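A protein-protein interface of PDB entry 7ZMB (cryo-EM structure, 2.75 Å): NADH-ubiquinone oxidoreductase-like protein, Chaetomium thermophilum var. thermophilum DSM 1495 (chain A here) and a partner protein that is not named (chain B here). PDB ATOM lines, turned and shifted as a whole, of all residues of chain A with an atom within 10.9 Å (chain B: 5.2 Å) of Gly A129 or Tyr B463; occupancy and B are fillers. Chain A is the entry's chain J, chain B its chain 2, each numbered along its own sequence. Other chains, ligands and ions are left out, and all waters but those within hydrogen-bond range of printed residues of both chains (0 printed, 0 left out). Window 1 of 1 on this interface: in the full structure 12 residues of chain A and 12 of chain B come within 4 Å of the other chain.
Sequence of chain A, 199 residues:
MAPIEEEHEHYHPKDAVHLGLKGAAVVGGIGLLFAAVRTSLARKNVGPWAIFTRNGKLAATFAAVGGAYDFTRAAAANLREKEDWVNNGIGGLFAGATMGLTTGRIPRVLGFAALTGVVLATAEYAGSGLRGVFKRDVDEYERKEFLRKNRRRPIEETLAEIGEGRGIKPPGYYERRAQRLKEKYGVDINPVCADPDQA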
ATOM      1  N   VAL A 119      19.795  -9.095  -1.221  1.00  0.00           N
ATOM      2  CA  VAL A 119      18.639  -9.044  -0.332  1.00  0.00           C
ATOM      3  C   VAL A 119      17.585  -8.101  -0.888  1.00  0.00           C
ATOM      4  O   VAL A 119      16.393  -8.427  -0.924  1.00  0.00           O
ATOM      5  CB  VAL A 119      19.066  -8.639   1.090  1.00  0.00           C
ATOM      6  CG1 VAL A 119      17.865  -8.159   1.889  1.00  0.00           C
ATOM      7  CG2 VAL A 119      19.747  -9.798   1.786  1.00  0.00           C
ATOM      8  N   THR A 122      15.793  -9.459  -3.990  1.00  0.00           N
ATOM      9  CA  THR A 122      14.858 -10.537  -3.704  1.00  0.00           C
ATOM     10  C   THR A 122      13.558 -10.004  -3.121  1.00  0.00           C
ATOM     11  O   THR A 122      12.468 -10.393  -3.552  1.00  0.00           O
ATOM     12  CB  THR A 122      15.505 -11.527  -2.744  1.00  0.00           C
ATOM     13  OG1 THR A 122      16.742 -11.988  -3.298  1.00  0.00           O
ATOM     14  CG2 THR A 122      14.598 -12.701  -2.506  1.00  0.00           C
ATOM     15  N   ALA A 123      13.651  -9.112  -2.135  1.00  0.00           N
ATOM     16  CA  ALA A 123      12.449  -8.594  -1.497  1.00  0.00           C
ATOM     17  C   ALA A 123      11.683  -7.636  -2.393  1.00  0.00           C
ATOM     18  O   ALA A 123      10.501  -7.384  -2.146  1.00  0.00           O
ATOM     19  CB  ALA A 123      12.805  -7.906  -0.182  1.00  0.00           C
ATOM     20  N   GLU A 124      12.318  -7.099  -3.426  1.00  0.00           N
ATOM     21  CA  GLU A 124      11.619  -6.220  -4.350  1.00  0.00           C
ATOM     22  C   GLU A 124      11.029  -6.965  -5.535  1.00  0.00           C
ATOM     23  O   GLU A 124      10.009  -6.535  -6.080  1.00  0.00           O
ATOM     24  CB  GLU A 124      12.557  -5.122  -4.847  1.00  0.00           C
ATOM     25  CG  GLU A 124      12.704  -3.922  -3.927  1.00  0.00           C
ATOM     26  CD  GLU A 124      13.070  -4.266  -2.486  1.00  0.00           C
ATOM     27  OE1 GLU A 124      14.079  -4.954  -2.248  1.00  0.00           O
ATOM     28  OE2 GLU A 124      12.380  -3.781  -1.576  1.00  0.00           O
ATOM     29  N   TYR A 125      11.643  -8.067  -5.953  1.00  0.00           N
ATOM     30  CA  TYR A 125      11.010  -8.891  -6.968  1.00  0.00           C
ATOM     31  C   TYR A 125       9.887  -9.740  -6.386  1.00  0.00           C
ATOM     32  O   TYR A 125       8.943 -10.088  -7.103  1.00  0.00           O
ATOM     33  CB  TYR A 125      12.044  -9.782  -7.653  1.00  0.00           C
ATOM     34  CG  TYR A 125      11.440 -10.623  -8.743  1.00  0.00           C
ATOM     35  CD1 TYR A 125      11.111 -10.063  -9.968  1.00  0.00           C
ATOM     36  CD2 TYR A 125      11.169 -11.969  -8.544  1.00  0.00           C
ATOM     37  CE1 TYR A 125      10.546 -10.820 -10.969  1.00  0.00           C
ATOM     38  CE2 TYR A 125      10.604 -12.736  -9.541  1.00  0.00           C
ATOM     39  CZ  TYR A 125      10.294 -12.154 -10.752  1.00  0.00           C
ATOM     40  OH  TYR A 125       9.729 -12.911 -11.752  1.00  0.00           O
ATOM     41  N   ALA A 126       9.966 -10.076  -5.101  1.00  0.00           N
ATOM     42  CA  ALA A 126       8.981 -10.941  -4.471  1.00  0.00           C
ATOM     43  C   ALA A 126       7.955 -10.186  -3.638  1.00  0.00           C
ATOM     44  O   ALA A 126       6.932 -10.771  -3.271  1.00  0.00           O
ATOM     45  CB  ALA A 126       9.679 -11.987  -3.592  1.00  0.00           C
ATOM     46  N   GLY A 127       8.189  -8.910  -3.340  1.00  0.00           N
ATOM     47  CA  GLY A 127       7.241  -8.152  -2.550  1.00  0.00           C
ATOM     48  C   GLY A 127       7.197  -8.575  -1.097  1.00  0.00           C
ATOM     49  O   GLY A 127       6.227  -9.202  -0.660  1.00  0.00           O
ATOM     50  N   SER A 128       8.257  -8.261  -0.351  1.00  0.00           N
ATOM     51  CA  SER A 128       8.335  -8.602   1.066  1.00  0.00           C
ATOM     52  C   SER A 128       7.079  -8.157   1.803  1.00  0.00           C
ATOM     53  O   SER A 128       6.669  -6.997   1.715  1.00  0.00           O
ATOM     54  CB  SER A 128       9.574  -7.951   1.686  1.00  0.00           C
ATOM     55  OG  SER A 128       9.639  -8.183   3.081  1.00  0.00           O
ATOM     56  N   GLY A 129       6.475  -9.088   2.538  1.00  0.00           N
ATOM     57  CA  GLY A 129       5.186  -8.863   3.160  1.00  0.00           C
ATOM     58  C   GLY A 129       5.207  -7.905   4.332  1.00  0.00           C
ATOM     59  O   GLY A 129       4.189  -7.733   5.009  1.00  0.00           O
ATOM     60  N   LEU A 130       6.347  -7.248   4.568  1.00  0.00           N
ATOM     61  CA  LEU A 130       6.457  -6.323   5.690  1.00  0.00           C
ATOM     62  C   LEU A 130       5.549  -5.110   5.533  1.00  0.00           C
ATOM     63  O   LEU A 130       5.367  -4.358   6.497  1.00  0.00           O
ATOM     64  CB  LEU A 130       7.909  -5.871   5.865  1.00  0.00           C
ATOM     65  CG  LEU A 130       8.976  -6.968   5.932  1.00  0.00           C
ATOM     66  CD1 LEU A 130      10.373  -6.361   5.983  1.00  0.00           C
ATOM     67  CD2 LEU A 130       8.751  -7.910   7.105  1.00  0.00           C
ATOM     68  N   ARG A 131       4.993  -4.893   4.345  1.00  0.00           N
ATOM     69  CA  ARG A 131       3.950  -3.899   4.108  1.00  0.00           C
ATOM     70  C   ARG A 131       2.764  -4.550   3.414  1.00  0.00           C
ATOM     71  O   ARG A 131       2.128  -3.976   2.526  1.00  0.00           O
ATOM     72  CB  ARG A 131       4.481  -2.724   3.296  1.00  0.00           C
ATOM     73  CG  ARG A 131       5.528  -1.909   4.026  1.00  0.00           C
ATOM     74  CD  ARG A 131       4.928  -1.226   5.242  1.00  0.00           C
ATOM     75  NE  ARG A 131       5.945  -0.547   6.037  1.00  0.00           N
ATOM     76  CZ  ARG A 131       5.680   0.262   7.057  1.00  0.00           C
ATOM     77  NH1 ARG A 131       6.669   0.842   7.717  1.00  0.00           N
ATOM     78  NH2 ARG A 131       4.427   0.502   7.406  1.00  0.00           N
ATOM     79  N   GLY A 132       2.455  -5.776   3.820  1.00  0.00           N
ATOM     80  CA  GLY A 132       1.388  -6.527   3.203  1.00  0.00           C
ATOM     81  C   GLY A 132       1.820  -7.117   1.871  1.00  0.00           C
ATOM     82  O   GLY A 132       2.964  -6.989   1.430  1.00  0.00           O
ATOM     83  N   VAL A 133       0.861  -7.776   1.225  1.00  0.00           N
ATOM     84  CA  VAL A 133       1.063  -8.394  -0.079  1.00  0.00           C
ATOM     85  C   VAL A 133      -0.082  -7.959  -0.987  1.00  0.00           C
ATOM     86  O   VAL A 133      -1.055  -7.346  -0.545  1.00  0.00           O
ATOM     87  CB  VAL A 133       1.142  -9.933   0.006  1.00  0.00           C
ATOM     88  CG1 VAL A 133       2.388 -10.371   0.777  1.00  0.00           C
ATOM     89  CG2 VAL A 133      -0.118 -10.492   0.649  1.00  0.00           C
ATOM     90  N   PHE A 134       0.052  -8.274  -2.273  1.00  0.00           N
ATOM     91  CA  PHE A 134      -0.948  -7.858  -3.248  1.00  0.00           C
ATOM     92  C   PHE A 134      -2.296  -8.498  -2.944  1.00  0.00           C
ATOM     93  O   PHE A 134      -2.392  -9.709  -2.732  1.00  0.00           O
ATOM     94  CB  PHE A 134      -0.493  -8.227  -4.660  1.00  0.00           C
ATOM     95  N   LYS A 135      -3.341  -7.675  -2.924  1.00  0.00           N
ATOM     96  CA  LYS A 135      -4.685  -8.178  -2.678  1.00  0.00           C
ATOM     97  C   LYS A 135      -5.196  -8.943  -3.892  1.00  0.00           C
ATOM     98  O   LYS A 135      -4.976  -8.539  -5.038  1.00  0.00           O
ATOM     99  CB  LYS A 135      -5.632  -7.026  -2.346  1.00  0.00           C
ATOM    100  N   ARG A 136      -5.876 -10.061  -3.635  1.00  0.00           N
ATOM    101  CA  ARG A 136      -6.391 -10.880  -4.727  1.00  0.00           C
ATOM    102  C   ARG A 136      -7.452 -10.132  -5.526  1.00  0.00           C
ATOM    103  O   ARG A 136      -7.368 -10.040  -6.757  1.00  0.00           O
ATOM    104  CB  ARG A 136      -6.955 -12.191  -4.176  1.00  0.00           C
ATOM    105  N   TYR B 313       2.443  -6.128  11.477  1.00  0.00           N
ATOM    106  CA  TYR B 313       3.774  -6.093  10.885  1.00  0.00           C
ATOM    107  C   TYR B 313       4.857  -6.266  11.935  1.00  0.00           C
ATOM    108  O   TYR B 313       5.955  -6.721  11.612  1.00  0.00           O
ATOM    109  CB  TYR B 313       3.999  -4.814  10.086  1.00  0.00           C
ATOM    110  CG  TYR B 313       3.015  -4.677   8.959  1.00  0.00           C
ATOM    111  CD1 TYR B 313       2.985  -5.605   7.933  1.00  0.00           C
ATOM    112  CD2 TYR B 313       2.178  -3.583   8.875  1.00  0.00           C
ATOM    113  CE1 TYR B 313       2.090  -5.486   6.893  1.00  0.00           C
ATOM    114  CE2 TYR B 313       1.289  -3.451   7.836  1.00  0.00           C
ATOM    115  CZ  TYR B 313       1.246  -4.403   6.847  1.00  0.00           C
ATOM    116  OH  TYR B 313       0.358  -4.261   5.810  1.00  0.00           O
ATOM    117  N   LEU B 316       5.532  -9.971  11.745  1.00  0.00           N
ATOM    118  CA  LEU B 316       6.488 -10.298  10.687  1.00  0.00           C
ATOM    119  C   LEU B 316       7.889  -9.825  11.013  1.00  0.00           C
ATOM    120  O   LEU B 316       8.861 -10.533  10.738  1.00  0.00           O
ATOM    121  CB  LEU B 316       6.058  -9.745   9.332  1.00  0.00           C
ATOM    122  CG  LEU B 316       4.813 -10.364   8.741  1.00  0.00           C
ATOM    123  CD1 LEU B 316       4.427  -9.644   7.484  1.00  0.00           C
ATOM    124  CD2 LEU B 316       5.169 -11.794   8.429  1.00  0.00           C
ATOM    125  N   LEU B 353       5.371 -16.343  11.752  1.00  0.00           N
ATOM    126  CA  LEU B 353       5.155 -16.227  10.315  1.00  0.00           C
ATOM    127  C   LEU B 353       3.808 -16.806   9.905  1.00  0.00           C
ATOM    128  O   LEU B 353       3.115 -16.234   9.059  1.00  0.00           O
ATOM    129  CB  LEU B 353       6.286 -16.922   9.560  1.00  0.00           C
ATOM    130  CG  LEU B 353       6.137 -17.016   8.043  1.00  0.00           C
ATOM    131  CD1 LEU B 353       6.157 -15.650   7.409  1.00  0.00           C
ATOM    132  CD2 LEU B 353       7.199 -17.907   7.460  1.00  0.00           C
ATOM    133  N   SER B 356       1.084 -14.404  11.034  1.00  0.00           N
ATOM    134  CA  SER B 356       1.028 -13.070  10.383  1.00  0.00           C
ATOM    135  C   SER B 356       0.414 -13.203   8.993  1.00  0.00           C
ATOM    136  O   SER B 356      -0.194 -12.231   8.520  1.00  0.00           O
ATOM    137  CB  SER B 356       2.369 -12.409  10.362  1.00  0.00           C
ATOM    138  OG  SER B 356       3.068 -12.627  11.572  1.00  0.00           O
ATOM    139  N   VAL B 357       0.621 -14.342   8.340  1.00  0.00           N
ATOM    140  CA  VAL B 357      -0.110 -14.586   7.072  1.00  0.00           C
ATOM    141  C   VAL B 357      -1.449 -15.092   7.602  1.00  0.00           C
ATOM    142  O   VAL B 357      -1.427 -16.082   8.319  1.00  0.00           O
ATOM    143  CB  VAL B 357       0.601 -15.687   6.268  1.00  0.00           C
ATOM    144  CG1 VAL B 357      -0.078 -15.984   4.943  1.00  0.00           C
ATOM    145  CG2 VAL B 357       2.086 -15.422   6.092  1.00  0.00           C
ATOM    146  N   ALA B 458       2.754 -19.779   3.364  1.00  0.00           N
ATOM    147  CA  ALA B 458       3.455 -18.509   3.086  1.00  0.00           C
ATOM    148  C   ALA B 458       3.736 -18.385   1.590  1.00  0.00           C
ATOM    149  O   ALA B 458       3.568 -17.282   1.053  1.00  0.00           O
ATOM    150  CB  ALA B 458       4.702 -18.445   3.925  1.00  0.00           C
ATOM    151  N   LEU B 459       4.133 -19.483   0.946  1.00  0.00           N
ATOM    152  CA  LEU B 459       4.416 -19.459  -0.508  1.00  0.00           C
ATOM    153  C   LEU B 459       3.134 -19.116  -1.261  1.00  0.00           C
ATOM    154  O   LEU B 459       3.207 -18.334  -2.216  1.00  0.00           O
ATOM    155  CB  LEU B 459       4.974 -20.814  -0.954  1.00  0.00           C
ATOM    156  CG  LEU B 459       6.479 -20.997  -0.785  1.00  0.00           C
ATOM    157  CD1 LEU B 459       6.874 -22.433  -1.079  1.00  0.00           C
ATOM    158  CD2 LEU B 459       7.244 -20.040  -1.682  1.00  0.00           C
ATOM    159  N   ASN B 461       0.625 -17.346  -0.174  1.00  0.00           N
ATOM    160  CA  ASN B 461       0.152 -15.957   0.034  1.00  0.00           C
ATOM    161  C   ASN B 461       1.174 -14.884  -0.350  1.00  0.00           C
ATOM    162  O   ASN B 461       0.966 -13.739   0.056  1.00  0.00           O
ATOM    163  CB  ASN B 461      -0.524 -15.745   1.390  1.00  0.00           C
ATOM    164  CG  ASN B 461      -2.016 -15.988   1.338  1.00  0.00           C
ATOM    165  OD1 ASN B 461      -2.491 -16.786   0.535  1.00  0.00           O
ATOM    166  ND2 ASN B 461      -2.762 -15.307   2.191  1.00  0.00           N
ATOM    167  N   GLY B 462       2.236 -15.245  -1.079  1.00  0.00           N
ATOM    168  CA  GLY B 462       3.151 -14.223  -1.618  1.00  0.00           C
ATOM    169  C   GLY B 462       4.284 -13.836  -0.682  1.00  0.00           C
ATOM    170  O   GLY B 462       5.067 -12.957  -1.059  1.00  0.00           O
ATOM    171  N   TYR B 463       4.379 -14.476   0.480  1.00  0.00           N
ATOM    172  CA  TYR B 463       5.483 -14.211   1.433  1.00  0.00           C
ATOM    173  C   TYR B 463       6.663 -15.063   0.975  1.00  0.00           C
ATOM    174  O   TYR B 463       7.113 -15.937   1.729  1.00  0.00           O
ATOM    175  CB  TYR B 463       5.011 -14.506   2.859  1.00  0.00           C
ATOM    176  CG  TYR B 463       3.889 -13.639   3.370  1.00  0.00           C
ATOM    177  CD1 TYR B 463       2.583 -13.842   2.961  1.00  0.00           C
ATOM    178  CD2 TYR B 463       4.131 -12.631   4.285  1.00  0.00           C
ATOM    179  CE1 TYR B 463       1.548 -13.052   3.432  1.00  0.00           C
ATOM    180  CE2 TYR B 463       3.107 -11.837   4.771  1.00  0.00           C
ATOM    181  CZ  TYR B 463       1.809 -12.048   4.343  1.00  0.00           C
ATOM    182  OH  TYR B 463       0.796 -11.269   4.817  1.00  0.00           O
ATOM    183  N   ILE B 464       7.161 -14.790  -0.227  1.00  0.00           N
ATOM    184  CA  ILE B 464       8.242 -15.621  -0.818  1.00  0.00           C
ATOM    185  C   ILE B 464       9.542 -15.255  -0.116  1.00  0.00           C
ATOM    186  O   ILE B 464      10.387 -16.144   0.056  1.00  0.00           O
ATOM    187  CB  ILE B 464       8.327 -15.384  -2.340  1.00  0.00           C
ATOM    188  CG1 ILE B 464       6.941 -15.289  -2.983  1.00  0.00           C
ATOM    189  CG2 ILE B 464       9.192 -16.438  -3.014  1.00  0.00           C
ATOM    190  CD1 ILE B 464       6.127 -16.558  -2.886  1.00  0.00           C
ATOM    191  N   PHE B 465       9.677 -13.990   0.283  1.00  0.00           N
ATOM    192  CA  PHE B 465      10.944 -13.588   0.878  1.00  0.00           C
ATOM    193  C   PHE B 465      11.129 -14.199   2.263  1.00  0.00           C
ATOM    194  O   PHE B 465      12.221 -14.670   2.594  1.00  0.00           O
ATOM    195  CB  PHE B 465      11.027 -12.062   0.929  1.00  0.00           C
ATOM    196  CG  PHE B 465      12.315 -11.543   1.475  1.00  0.00           C
ATOM    197  CD1 PHE B 465      13.411 -11.389   0.652  1.00  0.00           C
ATOM    198  CD2 PHE B 465      12.433 -11.204   2.812  1.00  0.00           C
ATOM    199  CE1 PHE B 465      14.602 -10.913   1.149  1.00  0.00           C
ATOM    200  CE2 PHE B 465      13.622 -10.730   3.313  1.00  0.00           C
ATOM    201  CZ  PHE B 465      14.708 -10.584   2.479  1.00  0.00           C
ATOM    202  N   LEU B 466      10.077 -14.194   3.086  1.00  0.00           N
ATOM    203  CA  LEU B 466      10.153 -14.829   4.400  1.00  0.00           C
ATOM    204  C   LEU B 466      10.329 -16.334   4.303  1.00  0.00           C
ATOM    205  O   LEU B 466      10.932 -16.941   5.192  1.00  0.00           O
ATOM    206  CB  LEU B 466       8.907 -14.513   5.231  1.00  0.00           C
ATOM    207  CG  LEU B 466       8.834 -13.197   6.010  1.00  0.00           C
ATOM    208  CD1 LEU B 466       9.903 -13.183   7.068  1.00  0.00           C
ATOM    209  CD2 LEU B 466       8.990 -12.002   5.099  1.00  0.00           C
ATOM    210  N   SER B 467       9.788 -16.959   3.257  1.00  0.00           N
ATOM    211  CA  SER B 467      10.030 -18.381   3.050  1.00  0.00           C
ATOM    212  C   SER B 467      11.503 -18.649   2.790  1.00  0.00           C
ATOM    213  O   SER B 467      12.052 -19.648   3.262  1.00  0.00           O
ATOM    214  CB  SER B 467       9.182 -18.898   1.895  1.00  0.00           C
ATOM    215  OG  SER B 467       7.844 -19.088   2.293  1.00  0.00           O
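Among the printed residues, merely in contact across the chains: Val A119 with Phe B465, Thr A122 with Phe B465, Ala A123 with Phe B465, Ala A126 with Gly B462, Ala A126 with Ile B464, Gly A127 with Gly B462, Gly A129 with Tyr B313, Gly A129 with Leu B316, Gly A129 with Tyr B463, Leu A130 with Tyr B313, Leu A130 with Leu B316, Arg A131 with Tyr B313, Val A133 with Asn B461 and Val A133 with Tyr B463.
The backbone carbonyl oxygen (O) of Tyr B463 sits at hydrogen-bond distance from the side-chain hydroxyl (OG) of Ser B467 (3.3 Å).
The backbone carbonyl oxygen of Ala A123 sits at hydrogen-bond distance from the backbone NH of Ser A128, 3.0 Å away.
N of Tyr B463 sits at hydrogen-bond distance from O of Ala B458, at 3.0 Å.
Of the 16 printed residues of chain A, 10 touch a printed residue of chain B.
Printed residues of chain A that touch a printed residue of chain B: Val A119, Thr A122, Ala A123, Ala A126, Gly A127, Gly A129, Leu A130, Arg A131, Gly A132 and Val A133.
Hydrophobic or aromatic side chains of chain A within 4 Å of the printed part of chain B: Ala A123, Ala A126, Leu A130 and Val A133.
Among the printed residues, 15 pairs touch across the chains.
Among the printed residues, no Asp or Glu carboxylate lies within 4 Å of a Lys or Arg side-chain nitrogen of the other chain.
The backbone NH of Gly A132 lies close to the side-chain hydroxyl of Tyr B313, 3.3 Å away.
Glu A124 touches none of the printed residues of chain B.
Of chain B, only Tyr B313 (3.6 Å), Leu B316 (3.1 Å) and Tyr B463 (3.97 Å) come within 4 Å of Gly A129.
Of the printed residues of chain B, Gly A132 touches Tyr B313 (3.1 Å).
Printed residues of chain B within 4 Å of Val A133: Asn B461 (3.5 Å) and Tyr B463 (3.9 Å).
Printed residues of chain A within 4 Å of Tyr B313: Gly A129, Leu A130, Arg A131 and Gly A132.
Ser B356 touches none of the printed residues of chain A.
No residue of chain A comes within 4 Å of Val B357.
Of the printed residues of chain A, Asn B461 touches Val A133.
Of chain A, only Ala A126 and Gly A127 come within 4 Å of Gly B462.
Printed residues of chain A within 4 Å of Tyr B463: Gly A129 (3.97 Å) and Val A133 (3.9 Å).
Printed residues of chain A within 4 Å of Ile B464: Ala A126 (3.9 Å).
No residue of chain A comes within 4 Å of Leu B466.
The nearest residue of chain A that does not touch Tyr B463 is Gly A132 (5.0 Å).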
